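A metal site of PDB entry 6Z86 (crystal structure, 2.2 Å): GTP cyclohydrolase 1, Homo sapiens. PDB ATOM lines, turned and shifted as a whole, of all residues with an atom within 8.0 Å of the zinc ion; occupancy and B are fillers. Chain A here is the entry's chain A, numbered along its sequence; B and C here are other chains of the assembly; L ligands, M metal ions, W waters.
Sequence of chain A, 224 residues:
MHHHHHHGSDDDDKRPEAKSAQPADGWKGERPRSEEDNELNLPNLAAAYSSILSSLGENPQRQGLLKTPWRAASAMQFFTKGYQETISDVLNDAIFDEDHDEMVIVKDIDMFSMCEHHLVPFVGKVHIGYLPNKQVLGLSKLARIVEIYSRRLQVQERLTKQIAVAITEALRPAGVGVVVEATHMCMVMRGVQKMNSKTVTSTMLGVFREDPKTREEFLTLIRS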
ATOM      1  N   MET A 114     -26.406  19.129   4.808  1.00  0.00           N
ATOM      2  CA  MET A 114     -25.259  18.273   4.656  1.00  0.00           C
ATOM      3  C   MET A 114     -24.366  18.406   5.871  1.00  0.00           C
ATOM      4  O   MET A 114     -23.986  19.526   6.220  1.00  0.00           O
ATOM      5  CB  MET A 114     -24.497  18.701   3.403  1.00  0.00           C
ATOM      6  CG  MET A 114     -23.430  17.737   2.966  1.00  0.00           C
ATOM      7  SD  MET A 114     -24.062  16.158   2.360  1.00  0.00           S
ATOM      8  CE  MET A 114     -25.292  16.659   1.241  1.00  0.00           C
ATOM      9  N   CYS A 115     -24.051  17.304   6.533  1.00  0.00           N
ATOM     10  CA  CYS A 115     -23.177  17.303   7.696  1.00  0.00           C
ATOM     11  C   CYS A 115     -21.770  17.740   7.256  1.00  0.00           C
ATOM     12  O   CYS A 115     -21.197  17.149   6.338  1.00  0.00           O
ATOM     13  CB  CYS A 115     -23.162  15.907   8.315  1.00  0.00           C
ATOM     14  SG  CYS A 115     -21.788  15.587   9.440  1.00  0.00           S
ATOM     15  N   GLU A 116     -21.233  18.799   7.870  1.00  0.00           N
ATOM     16  CA  GLU A 116     -19.905  19.278   7.500  1.00  0.00           C
ATOM     17  C   GLU A 116     -18.785  18.380   7.985  1.00  0.00           C
ATOM     18  O   GLU A 116     -17.655  18.546   7.528  1.00  0.00           O
ATOM     19  CB  GLU A 116     -19.676  20.727   7.951  1.00  0.00           C
ATOM     20  CG  GLU A 116     -19.484  20.888   9.449  1.00  0.00           C
ATOM     21  CD  GLU A 116     -19.358  22.322   9.919  1.00  0.00           C
ATOM     22  OE1 GLU A 116     -18.898  22.540  11.061  1.00  0.00           O
ATOM     23  OE2 GLU A 116     -19.689  23.232   9.131  1.00  0.00           O
ATOM     24  N   HIS A 117     -19.065  17.459   8.925  1.00  0.00           N
ATOM     25  CA  HIS A 117     -18.030  16.583   9.437  1.00  0.00           C
ATOM     26  C   HIS A 117     -17.808  15.335   8.573  1.00  0.00           C
ATOM     27  O   HIS A 117     -16.671  14.890   8.453  1.00  0.00           O
ATOM     28  CB  HIS A 117     -18.325  16.221  10.908  1.00  0.00           C
ATOM     29  CG  HIS A 117     -18.238  17.417  11.801  1.00  0.00           C
ATOM     30  ND1 HIS A 117     -17.017  17.883  12.301  1.00  0.00           N
ATOM     31  CD2 HIS A 117     -19.218  18.262  12.199  1.00  0.00           C
ATOM     32  CE1 HIS A 117     -17.296  18.964  13.004  1.00  0.00           C
ATOM     33  NE2 HIS A 117     -18.605  19.234  12.978  1.00  0.00           N
ATOM     34  N   HIS A 118     -18.867  14.773   7.973  1.00  0.00           N
ATOM     35  CA  HIS A 118     -18.731  13.561   7.172  1.00  0.00           C
ATOM     36  C   HIS A 118     -19.213  13.693   5.732  1.00  0.00           C
ATOM     37  O   HIS A 118     -19.037  12.733   4.955  1.00  0.00           O
ATOM     38  CB  HIS A 118     -19.479  12.378   7.805  1.00  0.00           C
ATOM     39  CG  HIS A 118     -19.021  12.018   9.183  1.00  0.00           C
ATOM     40  ND1 HIS A 118     -19.669  12.495  10.314  1.00  0.00           N
ATOM     41  CD2 HIS A 118     -18.012  11.200   9.560  1.00  0.00           C
ATOM     42  CE1 HIS A 118     -19.024  11.977  11.346  1.00  0.00           C
ATOM     43  NE2 HIS A 118     -18.004  11.213  10.941  1.00  0.00           N
ATOM     44  N   LEU A 119     -19.854  14.821   5.382  1.00  0.00           N
ATOM     45  CA  LEU A 119     -20.385  15.094   4.045  1.00  0.00           C
ATOM     46  C   LEU A 119     -21.483  14.094   3.658  1.00  0.00           C
ATOM     47  O   LEU A 119     -21.562  13.667   2.507  1.00  0.00           O
ATOM     48  CB  LEU A 119     -19.284  15.196   2.972  1.00  0.00           C
ATOM     49  CG  LEU A 119     -18.212  16.244   3.234  1.00  0.00           C
ATOM     50  CD1 LEU A 119     -17.187  16.268   2.139  1.00  0.00           C
ATOM     51  CD2 LEU A 119     -18.812  17.632   3.410  1.00  0.00           C
ATOM     52  N   VAL A 120     -22.321  13.760   4.638  1.00  0.00           N
ATOM     53  CA  VAL A 120     -23.462  12.872   4.522  1.00  0.00           C
ATOM     54  C   VAL A 120     -24.692  13.715   4.936  1.00  0.00           C
ATOM     55  O   VAL A 120     -24.572  14.598   5.788  1.00  0.00           O
ATOM     56  CB  VAL A 120     -23.255  11.637   5.419  1.00  0.00           C
ATOM     57  CG1 VAL A 120     -24.480  10.721   5.422  1.00  0.00           C
ATOM     58  CG2 VAL A 120     -22.026  10.847   4.980  1.00  0.00           C
ATOM     59  N   PRO A 121     -25.875  13.531   4.302  1.00  0.00           N
ATOM     60  CA  PRO A 121     -27.021  14.372   4.649  1.00  0.00           C
ATOM     61  C   PRO A 121     -27.555  14.260   6.074  1.00  0.00           C
ATOM     62  O   PRO A 121     -27.398  13.250   6.747  1.00  0.00           O
ATOM     63  CB  PRO A 121     -28.112  13.895   3.680  1.00  0.00           C
ATOM     64  CG  PRO A 121     -27.366  13.221   2.550  1.00  0.00           C
ATOM     65  CD  PRO A 121     -26.191  12.596   3.198  1.00  0.00           C
ATOM     66  N   PHE A 122     -28.175  15.333   6.526  1.00  0.00           N
ATOM     67  CA  PHE A 122     -28.982  15.349   7.731  1.00  0.00           C
ATOM     68  C   PHE A 122     -30.277  16.038   7.326  1.00  0.00           C
ATOM     69  O   PHE A 122     -30.258  17.089   6.672  1.00  0.00           O
ATOM     70  CB  PHE A 122     -28.290  15.922   8.974  1.00  0.00           C
ATOM     71  CG  PHE A 122     -28.062  17.412   9.082  1.00  0.00           C
ATOM     72  CD1 PHE A 122     -29.008  18.229   9.681  1.00  0.00           C
ATOM     73  CD2 PHE A 122     -26.834  17.963   8.762  1.00  0.00           C
ATOM     74  CE1 PHE A 122     -28.754  19.583   9.860  1.00  0.00           C
ATOM     75  CE2 PHE A 122     -26.600  19.314   8.928  1.00  0.00           C
ATOM     76  CZ  PHE A 122     -27.560  20.113   9.486  1.00  0.00           C
ATOM     77  N   GLN A 154     -23.127  22.084   7.014  1.00  0.00           N
ATOM     78  CA  GLN A 154     -23.629  22.575   8.272  1.00  0.00           C
ATOM     79  C   GLN A 154     -23.399  21.729   9.522  1.00  0.00           C
ATOM     80  O   GLN A 154     -22.959  20.587   9.474  1.00  0.00           O
ATOM     81  CB  GLN A 154     -25.171  22.789   8.117  1.00  0.00           C
ATOM     82  CG  GLN A 154     -25.559  24.088   7.433  1.00  0.00           C
ATOM     83  CD  GLN A 154     -25.324  25.313   8.291  1.00  0.00           C
ATOM     84  OE1 GLN A 154     -24.665  25.282   9.343  1.00  0.00           O
ATOM     85  NE2 GLN A 154     -25.861  26.410   7.861  1.00  0.00           N
ATOM     86  N   HIS A 184     -29.695  12.496  11.446  1.00  0.00           N
ATOM     87  CA  HIS A 184     -28.364  12.603  10.866  1.00  0.00           C
ATOM     88  C   HIS A 184     -28.012  11.211  10.334  1.00  0.00           C
ATOM     89  O   HIS A 184     -27.901  10.287  11.113  1.00  0.00           O
ATOM     90  CB  HIS A 184     -27.358  13.030  11.951  1.00  0.00           C
ATOM     91  CG  HIS A 184     -27.465  14.484  12.302  1.00  0.00           C
ATOM     92  ND1 HIS A 184     -26.420  15.365  12.065  1.00  0.00           N
ATOM     93  CD2 HIS A 184     -28.483  15.167  12.859  1.00  0.00           C
ATOM     94  CE1 HIS A 184     -26.841  16.544  12.479  1.00  0.00           C
ATOM     95  NE2 HIS A 184     -28.084  16.474  12.962  1.00  0.00           N
ATOM     96  N   MET A 185     -27.823  11.072   9.009  1.00  0.00           N
ATOM     97  CA  MET A 185     -27.479   9.788   8.418  1.00  0.00           C
ATOM     98  C   MET A 185     -26.143   9.256   8.880  1.00  0.00           C
ATOM     99  O   MET A 185     -25.954   8.029   8.893  1.00  0.00           O
ATOM    100  CB  MET A 185     -27.543   9.823   6.903  1.00  0.00           C
ATOM    101  CG  MET A 185     -28.687  10.612   6.382  1.00  0.00           C
ATOM    102  SD  MET A 185     -29.924   9.629   5.554  1.00  0.00           S
ATOM    103  CE  MET A 185     -30.506   8.591   6.931  1.00  0.00           C
ATOM    104  N   CYS A 186     -25.205  10.113   9.294  1.00  0.00           N
ATOM    105  CA  CYS A 186     -23.944   9.647   9.892  1.00  0.00           C
ATOM    106  C   CYS A 186     -24.186   8.863  11.182  1.00  0.00           C
ATOM    107  O   CYS A 186     -23.274   8.171  11.647  1.00  0.00           O
ATOM    108  CB  CYS A 186     -23.029  10.819  10.191  1.00  0.00           C
ATOM    109  SG  CYS A 186     -23.072  12.130   8.974  1.00  0.00           S
ATOM    110  N   MET A 187     -25.324   9.102  11.832  1.00  0.00           N
ATOM    111  CA  MET A 187     -25.680   8.434  13.052  1.00  0.00           C
ATOM    112  C   MET A 187     -26.533   7.208  12.809  1.00  0.00           C
ATOM    113  O   MET A 187     -26.614   6.392  13.712  1.00  0.00           O
ATOM    114  CB  MET A 187     -26.404   9.393  14.012  1.00  0.00           C
ATOM    115  CG  MET A 187     -25.500  10.525  14.549  1.00  0.00           C
ATOM    116  SD  MET A 187     -26.100  11.192  16.129  1.00  0.00           S
ATOM    117  CE  MET A 187     -27.519  12.211  15.553  1.00  0.00           C
ATOM    118  N   ARG A 190     -24.025   4.594   9.825  1.00  0.00           N
ATOM    119  CA  ARG A 190     -22.661   4.360  10.246  1.00  0.00           C
ATOM    120  C   ARG A 190     -22.415   4.884  11.678  1.00  0.00           C
ATOM    121  O   ARG A 190     -23.371   5.289  12.328  1.00  0.00           O
ATOM    122  CB  ARG A 190     -21.649   4.894   9.218  1.00  0.00           C
ATOM    123  CG  ARG A 190     -21.858   6.327   8.782  1.00  0.00           C
ATOM    124  CD  ARG A 190     -20.541   7.060   8.806  1.00  0.00           C
ATOM    125  NE  ARG A 190     -20.496   7.876  10.008  1.00  0.00           N
ATOM    126  CZ  ARG A 190     -19.534   7.875  10.906  1.00  0.00           C
ATOM    127  NH1 ARG A 190     -19.628   8.633  11.984  1.00  0.00           N
ATOM    128  NH2 ARG A 190     -18.462   7.132  10.722  1.00  0.00           N
ATOM    129  N   ARG B  71     -12.620  12.152   7.887  1.00  0.00           N
ATOM    130  CA  ARG B  71     -13.886  11.578   8.372  1.00  0.00           C
ATOM    131  C   ARG B  71     -14.801  11.198   7.190  1.00  0.00           C
ATOM    132  O   ARG B  71     -15.491  10.177   7.253  1.00  0.00           O
ATOM    133  CB  ARG B  71     -14.628  12.502   9.345  1.00  0.00           C
ATOM    134  CG  ARG B  71     -13.831  12.991  10.556  1.00  0.00           C
ATOM    135  CD  ARG B  71     -13.394  11.897  11.528  1.00  0.00           C
ATOM    136  NE  ARG B  71     -11.933  11.752  11.550  1.00  0.00           N
ATOM    137  CZ  ARG B  71     -11.149  12.100  12.575  1.00  0.00           C
ATOM    138  NH1 ARG B  71      -9.827  11.972  12.482  1.00  0.00           N
ATOM    139  NH2 ARG B  71     -11.677  12.564  13.698  1.00  0.00           N
ATOM    140  N   ALA B  75     -15.848   7.356   6.199  1.00  0.00           N
ATOM    141  CA  ALA B  75     -17.270   7.085   6.034  1.00  0.00           C
ATOM    142  C   ALA B  75     -17.514   6.404   4.691  1.00  0.00           C
ATOM    143  O   ALA B  75     -18.166   5.376   4.661  1.00  0.00           O
ATOM    144  CB  ALA B  75     -18.089   8.361   6.135  1.00  0.00           C
ATOM    145  N   LEU C 139     -22.829  15.314  18.284  1.00  0.00           N
ATOM    146  CA  LEU C 139     -24.092  14.601  18.512  1.00  0.00           C
ATOM    147  C   LEU C 139     -23.947  13.112  18.782  1.00  0.00           C
ATOM    148  O   LEU C 139     -24.607  12.601  19.690  1.00  0.00           O
ATOM    149  CB  LEU C 139     -25.078  14.816  17.355  1.00  0.00           C
ATOM    150  CG  LEU C 139     -25.466  16.259  17.081  1.00  0.00           C
ATOM    151  CD1 LEU C 139     -26.261  16.355  15.831  1.00  0.00           C
ATOM    152  CD2 LEU C 139     -26.167  16.886  18.273  1.00  0.00           C
ATOM    153  N   SER C 140     -23.112  12.417  18.016  1.00  0.00           N
ATOM    154  CA  SER C 140     -22.937  10.977  18.205  1.00  0.00           C
ATOM    155  C   SER C 140     -22.288  10.596  19.535  1.00  0.00           C
ATOM    156  O   SER C 140     -22.477   9.485  20.000  1.00  0.00           O
ATOM    157  CB  SER C 140     -22.148  10.360  17.043  1.00  0.00           C
ATOM    158  OG  SER C 140     -20.787  10.727  17.146  1.00  0.00           O
HETATM  159  O1  LIG L   1     -14.230  13.631  14.782  1.00  0.00           O
HETATM  160  C1  LIG L   1     -21.769  15.993  13.020  1.00  0.00           C
HETATM  161  C2  LIG L   1     -20.616  15.322  15.184  1.00  0.00           C
HETATM  162  O2  LIG L   1     -15.700  11.688  13.989  1.00  0.00           O
HETATM  163  C3  LIG L   1     -18.505  14.578  15.529  1.00  0.00           C
HETATM  164  N1  LIG L   1     -22.186  17.680  16.106  1.00  0.00           N
HETATM  165  C4  LIG L   1     -17.224  14.335  14.786  1.00  0.00           C
HETATM  166  C5  LIG L   1     -19.444  13.376  15.662  1.00  0.00           C
HETATM  167  N2  LIG L   1     -21.475  16.174  14.368  1.00  0.00           N
HETATM  168  C6  LIG L   1     -20.699  13.835  14.907  1.00  0.00           C
HETATM  169  O3  LIG L   1     -16.338   9.863  12.387  1.00  0.00           O
HETATM  170  C7  LIG L   1     -24.050  18.626  14.117  1.00  0.00           C
HETATM  171  O4  LIG L   1     -15.041   9.221  14.484  1.00  0.00           O
HETATM  172  N3  LIG L   1     -23.928  19.127  15.401  1.00  0.00           N
HETATM  173  O5  LIG L   1     -17.426  10.140  14.687  1.00  0.00           O
HETATM  174  O6  LIG L   1     -19.828   9.655  14.280  1.00  0.00           O
HETATM  175  N4  LIG L   1     -23.060  19.258  17.529  1.00  0.00           N
HETATM  176  C8  LIG L   1     -23.037  18.673  16.328  1.00  0.00           C
HETATM  177  O7  LIG L   1     -19.267  15.648  14.939  1.00  0.00           O
HETATM  178  C9  LIG L   1     -22.260  17.183  14.847  1.00  0.00           C
HETATM  179  C10 LIG L   1     -23.099  17.603  13.807  1.00  0.00           C
HETATM  180  C11 LIG L   1     -22.757  16.856  12.650  1.00  0.00           C
HETATM  181  O8  LIG L   1     -16.539  13.367  15.605  1.00  0.00           O
HETATM  182  O9  LIG L   1     -18.815   9.146  16.511  1.00  0.00           O
HETATM  183  O10 LIG L   1     -19.721  13.175  17.036  1.00  0.00           O
HETATM  184  O11 LIG L   1     -21.927  13.267  15.366  1.00  0.00           O
HETATM  185  O12 LIG L   1     -24.967  18.979  13.373  1.00  0.00           O
HETATM  186  O13 LIG L   1     -14.937  11.686  16.384  1.00  0.00           O
HETATM  187  O14 LIG L   1     -18.216   7.759  14.528  1.00  0.00           O
HETATM  188  P1  LIG L   1     -15.245  12.607  15.207  1.00  0.00           P
HETATM  189  P2  LIG L   1     -16.055  10.150  13.872  1.00  0.00           P
HETATM  190  P3  LIG L   1     -18.640   9.155  15.003  1.00  0.00           P
HETATM  191 ZN    ZN M   1     -21.754  13.531  10.385  1.00  0.00          ZN
HETATM  192  O   HOH W   1     -23.667  13.250  12.261  1.00  0.00           O
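The zinc ion is bound by the side-chain sulfur of Cys 115 (2.3 Å), a ring nitrogen (ND1) of His 118 (2.3 Å) and the side-chain sulfur of Cys 186 (2.4 Å). Slightly farther from the zinc ion lies water W1 (2.7 Å).
A ring nitrogen (NE2) of His 118 is in hydrogen-bond range of an oxygen (O3) of the ligand (2.6 Å). OG of Ser 140 of chain C sits at hydrogen-bond distance from O9 of the ligand (2.6 Å). NH1 of Arg 190 lies within salt-bridge range of O6 of the ligand (2.5 Å). A nitrogen (N1) of the ligand lies within hydrogen-bond range of the backbone NH of Leu 139 of chain C. NH2 of Arg 71 of chain B is in salt-bridge range of O1 of the ligand, at 3.0 Å. The backbone NH (N) of Ser 140 of chain C sits at hydrogen-bond distance from an oxygen (O11) of the ligand, at 3.0 Å.
Three residues have an atom within 4 Å of the zinc ion: Cys 115, His 118 and Cys 186. The nearest printed residue that does not touch the zinc ion is His 117 (4.4 Å).
The backbone carbonyl oxygen (O) of Cys 186 lies within hydrogen-bond range of the guanidinium group (NE) of Arg 190 (3.2 Å). SG of Cys 115 sits close to N of His 117. NE2 of His 118 sits at hydrogen-bond distance from NH1 of Arg 190, at 3.2 Å. The backbone carbonyl oxygen of Val 120 is in hydrogen-bond range of the backbone NH of Cys 115.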
